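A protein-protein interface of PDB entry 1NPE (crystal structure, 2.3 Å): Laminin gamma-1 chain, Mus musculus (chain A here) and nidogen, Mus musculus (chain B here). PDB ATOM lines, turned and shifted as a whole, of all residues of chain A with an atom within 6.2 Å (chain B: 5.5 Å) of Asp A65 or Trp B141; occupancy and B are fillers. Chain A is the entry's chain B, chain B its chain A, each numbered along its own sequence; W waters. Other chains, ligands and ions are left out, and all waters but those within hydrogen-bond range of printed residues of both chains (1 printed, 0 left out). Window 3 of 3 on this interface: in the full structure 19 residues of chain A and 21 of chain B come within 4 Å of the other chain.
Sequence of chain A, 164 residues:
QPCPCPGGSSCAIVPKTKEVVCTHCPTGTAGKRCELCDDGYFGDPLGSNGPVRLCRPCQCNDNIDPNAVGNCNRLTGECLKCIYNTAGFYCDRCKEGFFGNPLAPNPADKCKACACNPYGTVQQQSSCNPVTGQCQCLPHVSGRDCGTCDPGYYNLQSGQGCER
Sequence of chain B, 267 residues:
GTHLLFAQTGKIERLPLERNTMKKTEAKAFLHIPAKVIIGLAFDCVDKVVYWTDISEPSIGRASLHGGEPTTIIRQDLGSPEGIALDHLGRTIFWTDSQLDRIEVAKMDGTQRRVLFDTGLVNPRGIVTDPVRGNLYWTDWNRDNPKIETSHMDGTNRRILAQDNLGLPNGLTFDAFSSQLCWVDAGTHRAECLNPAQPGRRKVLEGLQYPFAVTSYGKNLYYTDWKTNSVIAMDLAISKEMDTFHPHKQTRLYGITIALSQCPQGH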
ATOM      1  N   ASN A  63     -11.369  12.505  10.395  1.00  0.00           N
ATOM      2  CA  ASN A  63     -12.623  12.314   9.680  1.00  0.00           C
ATOM      3  C   ASN A  63     -13.806  12.048  10.608  1.00  0.00           C
ATOM      4  O   ASN A  63     -14.745  11.324  10.252  1.00  0.00           O
ATOM      5  CB  ASN A  63     -12.494  11.219   8.614  1.00  0.00           C
ATOM      6  CG  ASN A  63     -11.548  11.606   7.481  1.00  0.00           C
ATOM      7  OD1 ASN A  63     -11.396  12.786   7.149  1.00  0.00           O
ATOM      8  ND2 ASN A  63     -10.916  10.608   6.877  1.00  0.00           N
ATOM      9  N   ILE A  64     -13.727  12.597  11.818  1.00  0.00           N
ATOM     10  CA  ILE A  64     -14.798  12.487  12.796  1.00  0.00           C
ATOM     11  C   ILE A  64     -15.121  13.894  13.275  1.00  0.00           C
ATOM     12  O   ILE A  64     -14.298  14.803  13.144  1.00  0.00           O
ATOM     13  CB  ILE A  64     -14.448  11.573  13.995  1.00  0.00           C
ATOM     14  CG1 ILE A  64     -13.077  11.922  14.579  1.00  0.00           C
ATOM     15  CG2 ILE A  64     -14.553  10.106  13.586  1.00  0.00           C
ATOM     16  CD1 ILE A  64     -12.783  11.189  15.889  1.00  0.00           C
ATOM     17  N   ASP A  65     -16.338  14.090  13.769  1.00  0.00           N
ATOM     18  CA  ASP A  65     -16.761  15.407  14.241  1.00  0.00           C
ATOM     19  C   ASP A  65     -16.498  15.545  15.739  1.00  0.00           C
ATOM     20  O   ASP A  65     -16.974  14.737  16.529  1.00  0.00           O
ATOM     21  CB  ASP A  65     -18.251  15.617  13.939  1.00  0.00           C
ATOM     22  CG  ASP A  65     -18.654  17.072  13.983  1.00  0.00           C
ATOM     23  OD1 ASP A  65     -18.421  17.725  15.018  1.00  0.00           O
ATOM     24  OD2 ASP A  65     -19.191  17.569  12.973  1.00  0.00           O
ATOM     25  N   PRO A  66     -15.741  16.580  16.144  1.00  0.00           N
ATOM     26  CA  PRO A  66     -15.415  16.823  17.560  1.00  0.00           C
ATOM     27  C   PRO A  66     -16.650  17.110  18.420  1.00  0.00           C
ATOM     28  O   PRO A  66     -16.584  17.007  19.642  1.00  0.00           O
ATOM     29  CB  PRO A  66     -14.499  18.056  17.507  1.00  0.00           C
ATOM     30  CG  PRO A  66     -13.956  18.045  16.108  1.00  0.00           C
ATOM     31  CD  PRO A  66     -15.146  17.619  15.288  1.00  0.00           C
ATOM     32  N   ASN A  67     -17.761  17.483  17.780  1.00  0.00           N
ATOM     33  CA  ASN A  67     -19.003  17.783  18.492  1.00  0.00           C
ATOM     34  C   ASN A  67     -19.871  16.538  18.698  1.00  0.00           C
ATOM     35  O   ASN A  67     -20.889  16.587  19.387  1.00  0.00           O
ATOM     36  CB  ASN A  67     -19.802  18.877  17.770  1.00  0.00           C
ATOM     37  CG  ASN A  67     -20.927  19.444  18.629  1.00  0.00           C
ATOM     38  OD1 ASN A  67     -20.678  20.015  19.692  1.00  0.00           O
ATOM     39  ND2 ASN A  67     -22.169  19.265  18.183  1.00  0.00           N
ATOM     40  N   ALA A  68     -19.460  15.423  18.104  1.00  0.00           N
ATOM     41  CA  ALA A  68     -20.189  14.168  18.246  1.00  0.00           C
ATOM     42  C   ALA A  68     -19.671  13.401  19.454  1.00  0.00           C
ATOM     43  O   ALA A  68     -18.581  13.679  19.950  1.00  0.00           O
ATOM     44  CB  ALA A  68     -20.028  13.321  16.989  1.00  0.00           C
ATOM     45  N   VAL A  69     -20.483  12.473  19.949  1.00  0.00           N
ATOM     46  CA  VAL A  69     -20.107  11.616  21.070  1.00  0.00           C
ATOM     47  C   VAL A  69     -20.061  10.195  20.503  1.00  0.00           C
ATOM     48  O   VAL A  69     -20.694   9.921  19.483  1.00  0.00           O
ATOM     49  CB  VAL A  69     -21.144  11.678  22.233  1.00  0.00           C
ATOM     50  CG1 VAL A  69     -21.075  13.023  22.927  1.00  0.00           C
ATOM     51  CG2 VAL A  69     -22.567  11.427  21.712  1.00  0.00           C
ATOM     52  N   ASN A  71     -17.535   8.679  19.085  1.00  0.00           N
ATOM     53  CA  ASN A  71     -16.776   8.685  17.846  1.00  0.00           C
ATOM     54  C   ASN A  71     -15.989   7.406  17.575  1.00  0.00           C
ATOM     55  O   ASN A  71     -15.839   7.028  16.418  1.00  0.00           O
ATOM     56  CB  ASN A  71     -15.867   9.904  17.780  1.00  0.00           C
ATOM     57  CG  ASN A  71     -16.585  11.118  17.241  1.00  0.00           C
ATOM     58  OD1 ASN A  71     -17.521  10.989  16.443  1.00  0.00           O
ATOM     59  ND2 ASN A  71     -16.169  12.303  17.675  1.00  0.00           N
ATOM     60  N   LYS A  81     -18.165   6.872  13.859  1.00  0.00           N
ATOM     61  CA  LYS A  81     -18.957   7.906  13.201  1.00  0.00           C
ATOM     62  C   LYS A  81     -18.147   8.739  12.206  1.00  0.00           C
ATOM     63  O   LYS A  81     -17.985   9.951  12.381  1.00  0.00           O
ATOM     64  CB  LYS A  81     -19.608   8.807  14.254  1.00  0.00           C
ATOM     65  CG  LYS A  81     -20.426   8.040  15.301  1.00  0.00           C
ATOM     66  CD  LYS A  81     -21.286   8.965  16.143  1.00  0.00           C
ATOM     67  CE  LYS A  81     -22.097   8.178  17.165  1.00  0.00           C
ATOM     68  NZ  LYS A  81     -22.984   9.064  17.991  1.00  0.00           N
ATOM     69  N   ILE A  83     -17.224  10.912   9.026  1.00  0.00           N
ATOM     70  CA  ILE A  83     -17.978  11.884   8.252  1.00  0.00           C
ATOM     71  C   ILE A  83     -17.322  12.119   6.894  1.00  0.00           C
ATOM     72  O   ILE A  83     -16.407  11.382   6.513  1.00  0.00           O
ATOM     73  CB  ILE A  83     -18.208  13.206   9.027  1.00  0.00           C
ATOM     74  CG1 ILE A  83     -16.882  13.846   9.434  1.00  0.00           C
ATOM     75  CG2 ILE A  83     -19.067  12.937  10.270  1.00  0.00           C
ATOM     76  CD1 ILE A  83     -17.029  15.292   9.900  1.00  0.00           C
ATOM     77  N   GLU B  82     -29.292  10.576  22.353  1.00  0.00           N
ATOM     78  CA  GLU B  82     -28.550  11.626  23.034  1.00  0.00           C
ATOM     79  C   GLU B  82     -29.346  12.678  23.785  1.00  0.00           C
ATOM     80  O   GLU B  82     -28.769  13.604  24.354  1.00  0.00           O
ATOM     81  CB  GLU B  82     -27.635  12.316  22.035  1.00  0.00           C
ATOM     82  CG  GLU B  82     -26.560  11.410  21.483  1.00  0.00           C
ATOM     83  CD  GLU B  82     -25.792  12.061  20.376  1.00  0.00           C
ATOM     84  OE1 GLU B  82     -25.584  13.288  20.427  1.00  0.00           O
ATOM     85  OE2 GLU B  82     -25.393  11.343  19.448  1.00  0.00           O
ATOM     86  N   ASN B 123     -28.456  15.515  12.934  1.00  0.00           N
ATOM     87  CA  ASN B 123     -27.795  15.447  14.233  1.00  0.00           C
ATOM     88  C   ASN B 123     -28.695  15.963  15.364  1.00  0.00           C
ATOM     89  O   ASN B 123     -28.332  16.893  16.084  1.00  0.00           O
ATOM     90  CB  ASN B 123     -26.463  16.214  14.217  1.00  0.00           C
ATOM     91  CG  ASN B 123     -25.280  15.349  13.766  1.00  0.00           C
ATOM     92  OD1 ASN B 123     -24.399  15.811  13.046  1.00  0.00           O
ATOM     93  ND2 ASN B 123     -25.249  14.105  14.211  1.00  0.00           N
ATOM     94  N   PRO B 124     -29.904  15.390  15.514  1.00  0.00           N
ATOM     95  CA  PRO B 124     -30.763  15.873  16.600  1.00  0.00           C
ATOM     96  C   PRO B 124     -30.056  15.548  17.909  1.00  0.00           C
ATOM     97  O   PRO B 124     -29.299  14.581  17.983  1.00  0.00           O
ATOM     98  CB  PRO B 124     -32.025  15.024  16.437  1.00  0.00           C
ATOM     99  CG  PRO B 124     -31.473  13.724  15.917  1.00  0.00           C
ATOM    100  CD  PRO B 124     -30.521  14.232  14.845  1.00  0.00           C
ATOM    101  N   ARG B 125     -30.285  16.353  18.934  1.00  0.00           N
ATOM    102  CA  ARG B 125     -29.638  16.102  20.208  1.00  0.00           C
ATOM    103  C   ARG B 125     -30.523  16.558  21.353  1.00  0.00           C
ATOM    104  O   ARG B 125     -31.201  15.739  21.963  1.00  0.00           O
ATOM    105  CB  ARG B 125     -28.247  16.765  20.241  1.00  0.00           C
ATOM    106  CG  ARG B 125     -27.536  16.717  21.585  1.00  0.00           C
ATOM    107  CD  ARG B 125     -26.081  17.132  21.446  1.00  0.00           C
ATOM    108  NE  ARG B 125     -25.252  16.037  20.960  1.00  0.00           N
ATOM    109  CZ  ARG B 125     -24.020  16.171  20.476  1.00  0.00           C
ATOM    110  NH1 ARG B 125     -23.447  17.370  20.385  1.00  0.00           N
ATOM    111  NH2 ARG B 125     -23.327  15.085  20.163  1.00  0.00           N
ATOM    112  N   THR B 139     -33.186  20.357  19.154  1.00  0.00           N
ATOM    113  CA  THR B 139     -32.100  20.969  18.395  1.00  0.00           C
ATOM    114  C   THR B 139     -31.529  19.924  17.450  1.00  0.00           C
ATOM    115  O   THR B 139     -31.646  18.720  17.690  1.00  0.00           O
ATOM    116  CB  THR B 139     -30.930  21.458  19.289  1.00  0.00           C
ATOM    117  OG1 THR B 139     -30.196  20.333  19.787  1.00  0.00           O
ATOM    118  CG2 THR B 139     -31.438  22.277  20.450  1.00  0.00           C
ATOM    119  N   ASP B 140     -30.953  20.395  16.354  1.00  0.00           N
ATOM    120  CA  ASP B 140     -30.311  19.528  15.376  1.00  0.00           C
ATOM    121  C   ASP B 140     -29.057  20.310  15.025  1.00  0.00           C
ATOM    122  O   ASP B 140     -29.125  21.337  14.357  1.00  0.00           O
ATOM    123  CB  ASP B 140     -31.194  19.324  14.136  1.00  0.00           C
ATOM    124  CG  ASP B 140     -30.595  18.325  13.132  1.00  0.00           C
ATOM    125  OD1 ASP B 140     -29.360  18.168  13.069  1.00  0.00           O
ATOM    126  OD2 ASP B 140     -31.367  17.701  12.380  1.00  0.00           O
ATOM    127  N   TRP B 141     -27.912  19.839  15.502  1.00  0.00           N
ATOM    128  CA  TRP B 141     -26.669  20.553  15.241  1.00  0.00           C
ATOM    129  C   TRP B 141     -26.042  20.351  13.868  1.00  0.00           C
ATOM    130  O   TRP B 141     -24.860  20.642  13.682  1.00  0.00           O
ATOM    131  CB  TRP B 141     -25.658  20.352  16.380  1.00  0.00           C
ATOM    132  CG  TRP B 141     -25.274  18.949  16.644  1.00  0.00           C
ATOM    133  CD1 TRP B 141     -25.875  18.087  17.510  1.00  0.00           C
ATOM    134  CD2 TRP B 141     -24.150  18.255  16.096  1.00  0.00           C
ATOM    135  NE1 TRP B 141     -25.191  16.897  17.546  1.00  0.00           N
ATOM    136  CE2 TRP B 141     -24.124  16.973  16.690  1.00  0.00           C
ATOM    137  CE3 TRP B 141     -23.156  18.594  15.166  1.00  0.00           C
ATOM    138  CZ2 TRP B 141     -23.139  16.022  16.385  1.00  0.00           C
ATOM    139  CZ3 TRP B 141     -22.171  17.644  14.856  1.00  0.00           C
ATOM    140  CH2 TRP B 141     -22.173  16.375  15.468  1.00  0.00           C
ATOM    141  N   ASN B 142     -26.856  19.885  12.918  1.00  0.00           N
ATOM    142  CA  ASN B 142     -26.486  19.678  11.502  1.00  0.00           C
ATOM    143  C   ASN B 142     -25.486  20.768  11.106  1.00  0.00           C
ATOM    144  O   ASN B 142     -25.854  21.935  10.994  1.00  0.00           O
ATOM    145  CB  ASN B 142     -27.766  19.825  10.654  1.00  0.00           C
ATOM    146  CG  ASN B 142     -27.560  19.555   9.155  1.00  0.00           C
ATOM    147  OD1 ASN B 142     -28.515  19.217   8.457  1.00  0.00           O
ATOM    148  ND2 ASN B 142     -26.343  19.725   8.659  1.00  0.00           N
ATOM    149  N   ARG B 143     -24.226  20.387  10.918  1.00  0.00           N
ATOM    150  CA  ARG B 143     -23.174  21.346  10.570  1.00  0.00           C
ATOM    151  C   ARG B 143     -23.563  22.351   9.491  1.00  0.00           C
ATOM    152  O   ARG B 143     -23.290  23.545   9.621  1.00  0.00           O
ATOM    153  CB  ARG B 143     -21.904  20.611  10.139  1.00  0.00           C
ATOM    154  CG  ARG B 143     -21.085  20.037  11.272  1.00  0.00           C
ATOM    155  CD  ARG B 143     -20.238  21.099  11.955  1.00  0.00           C
ATOM    156  NE  ARG B 143     -19.356  20.495  12.946  1.00  0.00           N
ATOM    157  CZ  ARG B 143     -18.592  21.171  13.800  1.00  0.00           C
ATOM    158  NH1 ARG B 143     -18.576  22.500  13.801  1.00  0.00           N
ATOM    159  NH2 ARG B 143     -17.874  20.508  14.689  1.00  0.00           N
ATOM    160  N   ASP B 144     -24.217  21.866   8.439  1.00  0.00           N
ATOM    161  CA  ASP B 144     -24.623  22.722   7.329  1.00  0.00           C
ATOM    162  C   ASP B 144     -25.902  23.519   7.549  1.00  0.00           C
ATOM    163  O   ASP B 144     -26.000  24.665   7.115  1.00  0.00           O
ATOM    164  CB  ASP B 144     -24.716  21.911   6.030  1.00  0.00           C
ATOM    165  CG  ASP B 144     -23.363  21.363   5.594  1.00  0.00           C
ATOM    166  OD1 ASP B 144     -22.432  22.172   5.386  1.00  0.00           O
ATOM    167  OD2 ASP B 144     -23.228  20.123   5.479  1.00  0.00           O
ATOM    168  N   PRO B 146     -27.986  23.947  10.902  1.00  0.00           N
ATOM    169  CA  PRO B 146     -28.392  23.781  12.303  1.00  0.00           C
ATOM    170  C   PRO B 146     -29.774  24.400  12.534  1.00  0.00           C
ATOM    171  O   PRO B 146     -30.130  25.385  11.893  1.00  0.00           O
ATOM    172  CB  PRO B 146     -27.304  24.547  13.057  1.00  0.00           C
ATOM    173  CG  PRO B 146     -26.959  25.645  12.099  1.00  0.00           C
ATOM    174  CD  PRO B 146     -26.867  24.898  10.791  1.00  0.00           C
ATOM    175  N   LYS B 147     -30.550  23.837  13.450  1.00  0.00           N
ATOM    176  CA  LYS B 147     -31.877  24.380  13.702  1.00  0.00           C
ATOM    177  C   LYS B 147     -32.501  24.018  15.041  1.00  0.00           C
ATOM    178  O   LYS B 147     -32.050  23.102  15.730  1.00  0.00           O
ATOM    179  CB  LYS B 147     -32.827  23.985  12.565  1.00  0.00           C
ATOM    180  CG  LYS B 147     -32.863  22.499  12.286  1.00  0.00           C
ATOM    181  CD  LYS B 147     -33.706  22.150  11.070  1.00  0.00           C
ATOM    182  CE  LYS B 147     -33.767  20.633  10.894  1.00  0.00           C
ATOM    183  NZ  LYS B 147     -34.696  20.198   9.810  1.00  0.00           N
ATOM    184  N   GLY B 167     -24.909  27.690  15.289  1.00  0.00           N
ATOM    185  CA  GLY B 167     -23.715  26.949  14.928  1.00  0.00           C
ATOM    186  C   GLY B 167     -23.849  25.500  15.350  1.00  0.00           C
ATOM    187  O   GLY B 167     -24.055  24.613  14.521  1.00  0.00           O
ATOM    188  N   LEU B 168     -23.723  25.256  16.648  1.00  0.00           N
ATOM    189  CA  LEU B 168     -23.850  23.921  17.198  1.00  0.00           C
ATOM    190  C   LEU B 168     -24.811  23.949  18.395  1.00  0.00           C
ATOM    191  O   LEU B 168     -24.375  23.987  19.553  1.00  0.00           O
ATOM    192  CB  LEU B 168     -22.473  23.389  17.622  1.00  0.00           C
ATOM    193  CG  LEU B 168     -21.382  23.280  16.544  1.00  0.00           C
ATOM    194  CD1 LEU B 168     -20.035  22.890  17.177  1.00  0.00           C
ATOM    195  CD2 LEU B 168     -21.782  22.270  15.474  1.00  0.00           C
ATOM    196  N   PRO B 169     -26.131  24.047  18.131  1.00  0.00           N
ATOM    197  CA  PRO B 169     -27.094  24.069  19.241  1.00  0.00           C
ATOM    198  C   PRO B 169     -27.150  22.672  19.848  1.00  0.00           C
ATOM    199  O   PRO B 169     -27.782  21.775  19.300  1.00  0.00           O
ATOM    200  CB  PRO B 169     -28.404  24.467  18.558  1.00  0.00           C
ATOM    201  CG  PRO B 169     -28.252  23.947  17.163  1.00  0.00           C
ATOM    202  CD  PRO B 169     -26.808  24.276  16.841  1.00  0.00           C
ATOM    203  N   ASN B 170     -26.431  22.484  20.952  1.00  0.00           N
ATOM    204  CA  ASN B 170     -26.359  21.185  21.604  1.00  0.00           C
ATOM    205  C   ASN B 170     -27.478  20.821  22.568  1.00  0.00           C
ATOM    206  O   ASN B 170     -27.849  19.662  22.679  1.00  0.00           O
ATOM    207  CB  ASN B 170     -24.997  21.016  22.274  1.00  0.00           C
ATOM    208  CG  ASN B 170     -23.884  20.780  21.267  1.00  0.00           C
ATOM    209  OD1 ASN B 170     -24.094  20.148  20.223  1.00  0.00           O
ATOM    210  ND2 ASN B 170     -22.694  21.275  21.575  1.00  0.00           N
HETATM  211  O   HOH W   1     -23.016  12.599  18.357  1.00  0.00           O
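Water W1 lies within hydrogen-bond range of OE2 of Glu B82 (2.9 Å), N of Val A69 (3.0 Å) and NH2 of Arg B125 (3.1 Å).
CZ3 of Trp B141 touches OD2 of Asp A65, at 3.5 Å.
Asn A67 touches Trp B141 (ND2 to CD2, 3.0 Å).
Arg B143 touches Asn A67 (NH2 to CB, 3.98 Å).
Asn A67 touches Leu B168 (CG to CD1, 3.8 Å).
Ala A68 touches Arg B125 (CA to NH2, 3.8 Å).
Ala A68 touches Trp B141 (N to CH2, 3.9 Å).
CD of Glu B82 touches CG2 of Val A69 (3.5 Å).
N of Val A69 touches NH2 of Arg B125, at 3.9 Å.
Of chain A, only Asp A65 (3.5 Å), Asn A67 (3.0 Å) and Ala A68 (3.9 Å) come within 4 Å of Trp B141.
Of the printed residues of chain A, Leu B168 touches Asn A67.
Printed residues of chain A within 4 Å of Glu B82: Val A69 and Lys A81.
Printed residues of chain B within 4 Å of Ala A68: Arg B125 and Trp B141.
Printed residues of chain A within 4 Å of Asn B170: Asn A67.
Printed residues of chain B within 4 Å of Lys A81: Glu B82.
Pro A66 touches none of the printed residues of chain B.
The nearest residue of chain A that does not touch Trp B141 is Val A69 (5.7 Å).
The backbone carbonyl oxygen of Val A69 sits at hydrogen-bond distance from the side-chain amino group of Lys A81, at 2.9 Å.
The backbone carbonyl oxygen (O) of Thr B139 lies within hydrogen-bond range of the backbone NH (N) of Arg B125, 3.0 Å away.
OD1 of Asp A65 is in hydrogen-bond range of N of Asn A67 (2.9 Å).
O of Asn B123 is in hydrogen-bond range of N of Trp B141.
The side-chain carboxylate (OE1) of Glu B82 is in salt-bridge range of the guanidinium group (NE) of Arg B125, at 2.8 Å.
The guanidinium group of Arg B125 sits at hydrogen-bond distance from the side-chain amide oxygen of Asn B170, 2.9 Å away.
Hydrophobic or aromatic side chains of chain A within 4 Å of the printed part of chain B: Val A69.
Of the 16 printed residues of chain B, 6 touch a printed residue of chain A.
Printed residues of chain B that touch a printed residue of chain A: Glu B82, Arg B125, Trp B141, Arg B143, Leu B168 and Asn B170.
Hydrophobic or aromatic side chains of chain B within 4 Å of the printed part of chain A: Trp B141 and Leu B168.
Among the printed residues, 12 pairs touch across the chains.
The side-chain amide nitrogen (ND2) of Asn A67 lies within hydrogen-bond range of the side-chain amide oxygen (OD1) of Asn B170, 2.9 Å away.
The side-chain carboxylate (OE2) of Glu B82 lies within salt-bridge range of the side-chain amino group (NZ) of Lys A81.
O of Asn A67 is in hydrogen-bond range of NH1 of Arg B125 (2.9 Å).
NH2 of Arg B143 lies within salt-bridge range of OD1 of Asp A65 (2.9 Å).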
